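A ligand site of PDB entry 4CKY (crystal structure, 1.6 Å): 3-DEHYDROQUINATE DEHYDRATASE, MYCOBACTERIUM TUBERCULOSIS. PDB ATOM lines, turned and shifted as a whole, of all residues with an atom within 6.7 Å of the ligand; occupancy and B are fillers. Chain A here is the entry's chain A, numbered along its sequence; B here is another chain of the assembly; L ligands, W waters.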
ATOM      1  N   PRO A  11      21.325 -29.282   3.225  1.00  0.00           N
ATOM      2  CA  PRO A  11      20.640 -27.998   3.375  1.00  0.00           C
ATOM      3  C   PRO A  11      21.237 -26.870   2.530  1.00  0.00           C
ATOM      4  O   PRO A  11      22.463 -26.734   2.379  1.00  0.00           O
ATOM      5  CB  PRO A  11      20.755 -27.682   4.864  1.00  0.00           C
ATOM      6  CG  PRO A  11      21.136 -28.902   5.518  1.00  0.00           C
ATOM      7  CD  PRO A  11      21.594 -29.920   4.530  1.00  0.00           C
ATOM      8  N   ASN A  12      20.309 -26.084   1.981  1.00  0.00           N
ATOM      9  CA  ASN A  12      20.558 -24.935   1.171  1.00  0.00           C
ATOM     10  C   ASN A  12      21.024 -25.215  -0.254  1.00  0.00           C
ATOM     11  O   ASN A  12      21.069 -24.299  -1.067  1.00  0.00           O
ATOM     12  CB  ASN A  12      21.523 -23.953   1.857  1.00  0.00           C
ATOM     13  CG  ASN A  12      21.018 -23.461   3.187  1.00  0.00           C
ATOM     14  OD1 ASN A  12      19.930 -22.930   3.275  1.00  0.00           O
ATOM     15  ND2 ASN A  12      21.775 -23.675   4.231  1.00  0.00           N
ATOM     16  N   LEU A  13      21.265 -26.476  -0.597  1.00  0.00           N
ATOM     17  CA  LEU A  13      21.690 -26.798  -1.948  1.00  0.00           C
ATOM     18  C   LEU A  13      20.565 -26.636  -2.971  1.00  0.00           C
ATOM     19  O   LEU A  13      20.833 -26.503  -4.186  1.00  0.00           O
ATOM     20  CB  LEU A  13      22.300 -28.198  -2.035  1.00  0.00           C
ATOM     21  CG  LEU A  13      23.831 -28.408  -1.807  1.00  0.00           C
ATOM     22  CD1 LEU A  13      24.756 -27.585  -2.729  1.00  0.00           C
ATOM     23  CD2 LEU A  13      24.243 -28.338  -0.388  1.00  0.00           C
ATOM     24  N   LEU A  16      20.982 -23.297  -5.026  1.00  0.00           N
ATOM     25  CA  LEU A  16      22.032 -23.100  -5.999  1.00  0.00           C
ATOM     26  C   LEU A  16      21.566 -22.178  -7.127  1.00  0.00           C
ATOM     27  O   LEU A  16      20.480 -22.344  -7.686  1.00  0.00           O
ATOM     28  CB  LEU A  16      22.437 -24.427  -6.618  1.00  0.00           C
ATOM     29  CG  LEU A  16      23.501 -25.235  -5.904  1.00  0.00           C
ATOM     30  CD1 LEU A  16      23.610 -26.638  -6.509  1.00  0.00           C
ATOM     31  CD2 LEU A  16      24.844 -24.514  -5.917  1.00  0.00           C
ATOM     32  N   ASN A  75      27.074 -34.081  -0.633  1.00  0.00           N
ATOM     33  CA  ASN A  75      27.396 -32.716  -0.266  1.00  0.00           C
ATOM     34  C   ASN A  75      26.408 -32.336   0.815  1.00  0.00           C
ATOM     35  O   ASN A  75      25.256 -31.971   0.509  1.00  0.00           O
ATOM     36  CB  ASN A  75      27.297 -31.780  -1.466  1.00  0.00           C
ATOM     37  CG  ASN A  75      27.687 -30.364  -1.106  1.00  0.00           C
ATOM     38  OD1 ASN A  75      27.858 -30.028   0.087  1.00  0.00           O
ATOM     39  ND2 ASN A  75      27.824 -29.516  -2.128  1.00  0.00           N
ATOM     40  N   ALA A  76      26.839 -32.466   2.062  1.00  0.00           N
ATOM     41  CA  ALA A  76      25.927 -32.285   3.216  1.00  0.00           C
ATOM     42  C   ALA A  76      25.706 -30.820   3.606  1.00  0.00           C
ATOM     43  O   ALA A  76      25.004 -30.529   4.579  1.00  0.00           O
ATOM     44  CB  ALA A  76      26.449 -33.070   4.406  1.00  0.00           C
ATOM     45  N   GLY A  77      26.252 -29.888   2.846  1.00  0.00           N
ATOM     46  CA  GLY A  77      26.138 -28.471   3.211  1.00  0.00           C
ATOM     47  C   GLY A  77      26.661 -28.235   4.620  1.00  0.00           C
ATOM     48  O   GLY A  77      27.683 -28.793   5.024  1.00  0.00           O
ATOM     49  N   GLY A  78      26.004 -27.359   5.370  1.00  0.00           N
ATOM     50  CA  GLY A  78      26.502 -26.988   6.695  1.00  0.00           C
ATOM     51  C   GLY A  78      26.554 -28.149   7.668  1.00  0.00           C
ATOM     52  O   GLY A  78      27.319 -28.106   8.647  1.00  0.00           O
ATOM     53  N   LEU A  79      25.776 -29.203   7.420  1.00  0.00           N
ATOM     54  CA  LEU A  79      25.789 -30.373   8.307  1.00  0.00           C
ATOM     55  C   LEU A  79      27.137 -31.087   8.275  1.00  0.00           C
ATOM     56  O   LEU A  79      27.451 -31.856   9.187  1.00  0.00           O
ATOM     57  CB  LEU A  79      24.682 -31.350   7.955  1.00  0.00           C
ATOM     58  CG  LEU A  79      23.261 -30.817   8.006  1.00  0.00           C
ATOM     59  CD1 LEU A  79      22.280 -31.862   7.504  1.00  0.00           C
ATOM     60  CD2 LEU A  79      22.888 -30.381   9.395  1.00  0.00           C
ATOM     61  N   THR A  80      27.916 -30.884   7.210  1.00  0.00           N
ATOM     62  CA  THR A  80      29.281 -31.409   7.134  1.00  0.00           C
ATOM     63  C   THR A  80      30.060 -31.126   8.427  1.00  0.00           C
ATOM     64  O   THR A  80      30.847 -31.947   8.918  1.00  0.00           O
ATOM     65  CB  THR A  80      29.993 -30.763   5.936  1.00  0.00           C
ATOM     66  OG1 THR A  80      29.199 -30.943   4.740  1.00  0.00           O
ATOM     67  CG2 THR A  80      31.316 -31.369   5.734  1.00  0.00           C
ATOM     68  N   HIS A  81      29.887 -29.910   8.912  1.00  0.00           N
ATOM     69  CA  HIS A  81      30.690 -29.354   9.972  1.00  0.00           C
ATOM     70  C   HIS A  81      30.117 -29.618  11.361  1.00  0.00           C
ATOM     71  O   HIS A  81      30.801 -29.357  12.357  1.00  0.00           O
ATOM     72  CB  HIS A  81      30.890 -27.851   9.770  1.00  0.00           C
ATOM     73  CG  HIS A  81      31.246 -27.470   8.382  1.00  0.00           C
ATOM     74  ND1 HIS A  81      32.388 -27.916   7.755  1.00  0.00           N
ATOM     75  CD2 HIS A  81      30.556 -26.769   7.443  1.00  0.00           C
ATOM     76  CE1 HIS A  81      32.401 -27.480   6.507  1.00  0.00           C
ATOM     77  NE2 HIS A  81      31.295 -26.795   6.302  1.00  0.00           N
ATOM     78  N   VAL A 100      31.688 -34.186  -1.462  1.00  0.00           N
ATOM     79  CA  VAL A 100      31.917 -33.108  -2.426  1.00  0.00           C
ATOM     80  C   VAL A 100      31.478 -31.779  -1.834  1.00  0.00           C
ATOM     81  O   VAL A 100      30.413 -31.716  -1.222  1.00  0.00           O
ATOM     82  CB  VAL A 100      31.114 -33.359  -3.726  1.00  0.00           C
ATOM     83  CG1 VAL A 100      31.127 -32.146  -4.652  1.00  0.00           C
ATOM     84  CG2 VAL A 100      31.637 -34.597  -4.417  1.00  0.00           C
ATOM     85  N   HIS A 101      32.334 -30.764  -1.962  1.00  0.00           N
ATOM     86  CA  HIS A 101      31.963 -29.358  -1.728  1.00  0.00           C
ATOM     87  C   HIS A 101      32.250 -28.557  -2.985  1.00  0.00           C
ATOM     88  O   HIS A 101      33.330 -28.699  -3.617  1.00  0.00           O
ATOM     89  CB  HIS A 101      32.702 -28.800  -0.518  1.00  0.00           C
ATOM     90  CG  HIS A 101      32.386 -29.574   0.714  1.00  0.00           C
ATOM     91  ND1 HIS A 101      31.126 -29.549   1.278  1.00  0.00           N
ATOM     92  CD2 HIS A 101      33.062 -30.546   1.360  1.00  0.00           C
ATOM     93  CE1 HIS A 101      31.088 -30.405   2.284  1.00  0.00           C
ATOM     94  NE2 HIS A 101      32.248 -31.022   2.350  1.00  0.00           N
ATOM     95  N   ILE A 102      31.270 -27.737  -3.355  1.00  0.00           N
ATOM     96  CA  ILE A 102      31.400 -26.848  -4.506  1.00  0.00           C
ATOM     97  C   ILE A 102      32.516 -25.795  -4.298  1.00  0.00           C
ATOM     98  O   ILE A 102      33.375 -25.585  -5.177  1.00  0.00           O
ATOM     99  CB  ILE A 102      30.014 -26.217  -4.825  1.00  0.00           C
ATOM    100  CG1 ILE A 102      29.059 -27.334  -5.254  1.00  0.00           C
ATOM    101  CG2 ILE A 102      30.118 -25.140  -5.840  1.00  0.00           C
ATOM    102  CD1 ILE A 102      27.606 -26.908  -5.247  1.00  0.00           C
ATOM    103  N   SER A 103      32.474 -25.138  -3.140  1.00  0.00           N
ATOM    104  CA  SER A 103      33.433 -24.116  -2.754  1.00  0.00           C
ATOM    105  C   SER A 103      34.657 -24.769  -2.131  1.00  0.00           C
ATOM    106  O   SER A 103      34.638 -25.915  -1.686  1.00  0.00           O
ATOM    107  CB  SER A 103      32.806 -23.114  -1.752  1.00  0.00           C
ATOM    108  OG  SER A 103      32.575 -23.685  -0.474  1.00  0.00           O
ATOM    109  N   ASN A 104      35.744 -24.012  -2.120  1.00  0.00           N
ATOM    110  CA  ASN A 104      36.943 -24.433  -1.410  1.00  0.00           C
ATOM    111  C   ASN A 104      36.784 -23.998   0.036  1.00  0.00           C
ATOM    112  O   ASN A 104      37.080 -22.854   0.396  1.00  0.00           O
ATOM    113  CB  ASN A 104      38.216 -23.880  -2.038  1.00  0.00           C
ATOM    114  CG  ASN A 104      39.463 -24.369  -1.324  1.00  0.00           C
ATOM    115  OD1 ASN A 104      39.380 -25.022  -0.271  1.00  0.00           O
ATOM    116  ND2 ASN A 104      40.632 -24.097  -1.905  1.00  0.00           N
ATOM    117  N   VAL A 105      36.331 -24.935   0.867  1.00  0.00           N
ATOM    118  CA  VAL A 105      36.101 -24.669   2.274  1.00  0.00           C
ATOM    119  C   VAL A 105      37.358 -24.224   3.042  1.00  0.00           C
ATOM    120  O   VAL A 105      37.265 -23.608   4.084  1.00  0.00           O
ATOM    121  CB  VAL A 105      35.474 -25.897   2.976  1.00  0.00           C
ATOM    122  CG1 VAL A 105      34.075 -26.162   2.411  1.00  0.00           C
ATOM    123  CG2 VAL A 105      36.357 -27.142   2.852  1.00  0.00           C
ATOM    124  N   ARG A 108      37.875 -20.283   3.378  1.00  0.00           N
ATOM    125  CA  ARG A 108      36.774 -19.577   4.062  1.00  0.00           C
ATOM    126  C   ARG A 108      37.036 -19.552   5.587  1.00  0.00           C
ATOM    127  O   ARG A 108      38.204 -19.553   6.005  1.00  0.00           O
ATOM    128  CB  ARG A 108      35.445 -20.229   3.665  1.00  0.00           C
ATOM    129  CG  ARG A 108      35.269 -20.321   2.156  1.00  0.00           C
ATOM    130  CD  ARG A 108      33.931 -20.909   1.729  1.00  0.00           C
ATOM    131  NE  ARG A 108      32.802 -20.125   2.264  1.00  0.00           N
ATOM    132  CZ  ARG A 108      31.528 -20.463   2.116  1.00  0.00           C
ATOM    133  NH1 ARG A 108      31.173 -21.594   1.507  1.00  0.00           N
ATOM    134  NH2 ARG A 108      30.607 -19.667   2.610  1.00  0.00           N
ATOM    135  N   PHE A 111      36.005 -22.588  10.818  1.00  0.00           N
ATOM    136  CA  PHE A 111      35.073 -23.658  11.160  1.00  0.00           C
ATOM    137  C   PHE A 111      34.702 -24.599   9.988  1.00  0.00           C
ATOM    138  O   PHE A 111      34.306 -25.739  10.213  1.00  0.00           O
ATOM    139  CB  PHE A 111      33.831 -23.133  11.887  1.00  0.00           C
ATOM    140  CG  PHE A 111      32.924 -22.257  11.068  1.00  0.00           C
ATOM    141  CD1 PHE A 111      32.048 -22.808  10.149  1.00  0.00           C
ATOM    142  CD2 PHE A 111      32.887 -20.874  11.270  1.00  0.00           C
ATOM    143  CE1 PHE A 111      31.191 -22.003   9.420  1.00  0.00           C
ATOM    144  CE2 PHE A 111      32.019 -20.084  10.516  1.00  0.00           C
ATOM    145  CZ  PHE A 111      31.207 -20.652   9.591  1.00  0.00           C
ATOM    146  N   ARG A 112      34.795 -24.080   8.763  1.00  0.00           N
ATOM    147  CA  ARG A 112      34.517 -24.893   7.586  1.00  0.00           C
ATOM    148  C   ARG A 112      35.619 -25.865   7.225  1.00  0.00           C
ATOM    149  O   ARG A 112      35.415 -26.714   6.335  1.00  0.00           O
ATOM    150  CB  ARG A 112      34.211 -24.004   6.387  1.00  0.00           C
ATOM    151  CG  ARG A 112      32.985 -23.136   6.602  1.00  0.00           C
ATOM    152  CD  ARG A 112      32.587 -22.399   5.331  1.00  0.00           C
ATOM    153  NE  ARG A 112      31.646 -21.345   5.656  1.00  0.00           N
ATOM    154  CZ  ARG A 112      30.336 -21.524   5.773  1.00  0.00           C
ATOM    155  NH1 ARG A 112      29.784 -22.714   5.529  1.00  0.00           N
ATOM    156  NH2 ARG A 112      29.555 -20.498   6.090  1.00  0.00           N
ATOM    157  N   GLY A 127      36.181 -27.487  -3.971  1.00  0.00           N
ATOM    158  CA  GLY A 127      36.622 -26.315  -4.684  1.00  0.00           C
ATOM    159  C   GLY A 127      36.643 -26.373  -6.208  1.00  0.00           C
ATOM    160  O   GLY A 127      37.034 -25.382  -6.863  1.00  0.00           O
ATOM    161  N   TYR A 133      31.093 -33.032  -8.693  1.00  0.00           N
ATOM    162  CA  TYR A 133      30.113 -34.109  -8.767  1.00  0.00           C
ATOM    163  C   TYR A 133      30.395 -35.076  -9.932  1.00  0.00           C
ATOM    164  O   TYR A 133      30.267 -36.292  -9.795  1.00  0.00           O
ATOM    165  CB  TYR A 133      28.678 -33.581  -8.894  1.00  0.00           C
ATOM    166  CG  TYR A 133      28.126 -32.846  -7.699  1.00  0.00           C
ATOM    167  CD1 TYR A 133      27.474 -33.532  -6.680  1.00  0.00           C
ATOM    168  CD2 TYR A 133      28.232 -31.474  -7.616  1.00  0.00           C
ATOM    169  CE1 TYR A 133      26.907 -32.843  -5.607  1.00  0.00           C
ATOM    170  CE2 TYR A 133      27.697 -30.763  -6.556  1.00  0.00           C
ATOM    171  CZ  TYR A 133      27.033 -31.464  -5.530  1.00  0.00           C
ATOM    172  OH  TYR A 133      26.485 -30.756  -4.498  1.00  0.00           O
ATOM    173  N   VAL B  84      25.429 -24.304  11.339  1.00  0.00           N
ATOM    174  CA  VAL B  84      26.046 -23.661  10.169  1.00  0.00           C
ATOM    175  C   VAL B  84      25.032 -23.550   9.035  1.00  0.00           C
ATOM    176  O   VAL B  84      25.016 -22.540   8.309  1.00  0.00           O
ATOM    177  CB  VAL B  84      27.327 -24.407   9.722  1.00  0.00           C
ATOM    178  CG1 VAL B  84      27.871 -23.803   8.429  1.00  0.00           C
ATOM    179  CG2 VAL B  84      28.380 -24.334  10.810  1.00  0.00           C
ATOM    180  N   ALA B  85      24.173 -24.551   8.871  1.00  0.00           N
ATOM    181  CA  ALA B  85      23.119 -24.477   7.852  1.00  0.00           C
ATOM    182  C   ALA B  85      22.258 -23.188   7.990  1.00  0.00           C
ATOM    183  O   ALA B  85      21.960 -22.522   6.980  1.00  0.00           O
ATOM    184  CB  ALA B  85      22.239 -25.739   7.863  1.00  0.00           C
ATOM    185  N   ASP B  88      24.246 -20.155   6.871  1.00  0.00           N
ATOM    186  CA  ASP B  88      24.334 -20.126   5.413  1.00  0.00           C
ATOM    187  C   ASP B  88      23.065 -19.563   4.754  1.00  0.00           C
ATOM    188  O   ASP B  88      23.129 -18.746   3.831  1.00  0.00           O
ATOM    189  CB  ASP B  88      24.457 -21.588   4.826  1.00  0.00           C
ATOM    190  CG  ASP B  88      25.795 -22.356   5.156  1.00  0.00           C
ATOM    191  OD1 ASP B  88      26.885 -21.734   5.329  1.00  0.00           O
ATOM    192  OD2 ASP B  88      25.753 -23.624   5.166  1.00  0.00           O
HETATM  193  O1  LIG L   1      30.724 -25.489  -0.951  1.00  0.00           O
HETATM  194  C1  LIG L   1      29.877 -26.327  -0.616  1.00  0.00           C
HETATM  195  O2  LIG L   1      29.419 -27.263  -1.324  1.00  0.00           O
HETATM  196  C2  LIG L   1      29.286 -26.230   0.817  1.00  0.00           C
HETATM  197  O3  LIG L   1      28.787 -27.574   1.192  1.00  0.00           O
HETATM  198  C3  LIG L   1      30.343 -25.767   1.818  1.00  0.00           C
HETATM  199  C4  LIG L   1      29.756 -25.699   3.228  1.00  0.00           C
HETATM  200  O4  LIG L   1      30.768 -25.169   4.172  1.00  0.00           O
HETATM  201  C5  LIG L   1      28.541 -24.819   3.288  1.00  0.00           C
HETATM  202  O5  LIG L   1      27.988 -24.938   4.636  1.00  0.00           O
HETATM  203  C6  LIG L   1      27.609 -25.154   2.222  1.00  0.00           C
HETATM  204  O6  LIG L   1      26.394 -25.233   2.480  1.00  0.00           O
HETATM  205  C7  LIG L   1      28.070 -25.243   0.863  1.00  0.00           C
HETATM  206  C8  LIG L   1      28.464 -23.790   0.354  1.00  0.00           C
HETATM  207  C9  LIG L   1      26.961 -25.797  -0.098  1.00  0.00           C
HETATM  208  O   HOH W   1      24.068 -25.453   4.324  1.00  0.00           O
HETATM  209  O   HOH W   2      29.138 -20.652  -0.912  1.00  0.00           O
HETATM  210  O   HOH W   3      24.631 -23.011   1.235  1.00  0.00           O
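Leu 13 touches the ligand (CD2 to C9, 3.7 Å). Gly 77 touches the ligand (CA to O6, 3.3 Å). CG1 of Val 105 touches C3 of the ligand, 3.8 Å away. Arg 108 touches the ligand (NH1 to C8, 3.7 Å). Val 84 of chain B touches the ligand (CG1 to O5, 3.96 Å). Hydrophobic or aromatic side chains within 4 Å of the ligand: Leu 13, His 81, His 101, Ile 102, Val 105 and Val 84 of chain B. Within 4 Å of the ligand: Leu 13, Asn 75, Gly 77, Gly 78, His 81, His 101, Ile 102, Ser 103, Val 105, Arg 108, Arg 112, Val 84 of chain B and Asp 88 of chain B. Along chain A the residues within 4 Å of the ligand span positions 13 to 112. The nearest printed residue that does not touch the ligand is Pro 11 (4.2 Å).
An oxygen (O4) of the ligand lies within hydrogen-bond range of a ring nitrogen (NE2) of His 81 (2.7 Å). An oxygen (O4) of the ligand is in hydrogen-bond range of the guanidinium group of Arg 112 (3.0 Å). An oxygen (O5) of the ligand sits at hydrogen-bond distance from the backbone NH (N) of Gly 78. ND1 of His 101 lies within hydrogen-bond range of O3 of the ligand, at 3.1 Å. The side-chain carboxylate of Asp 88 of chain B lies within hydrogen-bond range of an oxygen (O5) of the ligand. An oxygen (O2) of the ligand is in hydrogen-bond range of the backbone NH of Ile 102, at 2.8 Å. OG of Ser 103 lies within hydrogen-bond range of O1 of the ligand. O1 of the ligand lies within hydrogen-bond range of N of Ser 103, 2.8 Å away. The side-chain amide oxygen of Asn 75 lies within hydrogen-bond range of an oxygen (O3) of the ligand (2.8 Å).
The side-chain amide oxygen of Asn 75 lies close to the backbone carbonyl oxygen of Val 100 (3.3 Å). The backbone NH (N) of Gly 127 is in hydrogen-bond range of the backbone carbonyl oxygen (O) of His 101 (3.1 Å). The backbone carbonyl oxygen (O) of Ser 103 lies within hydrogen-bond range of the backbone NH (N) of Gly 127 (3.2 Å). OH of Tyr 133 is in hydrogen-bond range of ND2 of Asn 75 (3.0 Å). The backbone carbonyl oxygen of Gly 77 is in hydrogen-bond range of the side-chain hydroxyl of Thr 80 (2.6 Å). The side-chain amide oxygen (OD1) of Asn 75 lies close to the backbone NH (N) of Gly 77, at 3.2 Å. The side-chain carboxylate (OD1) of Asp 88 of chain B lies within salt-bridge range of the guanidinium group (NH2) of Arg 112 (3.0 Å). OG of Ser 103 is in hydrogen-bond range of NH1 of Arg 108, 3.2 Å away.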
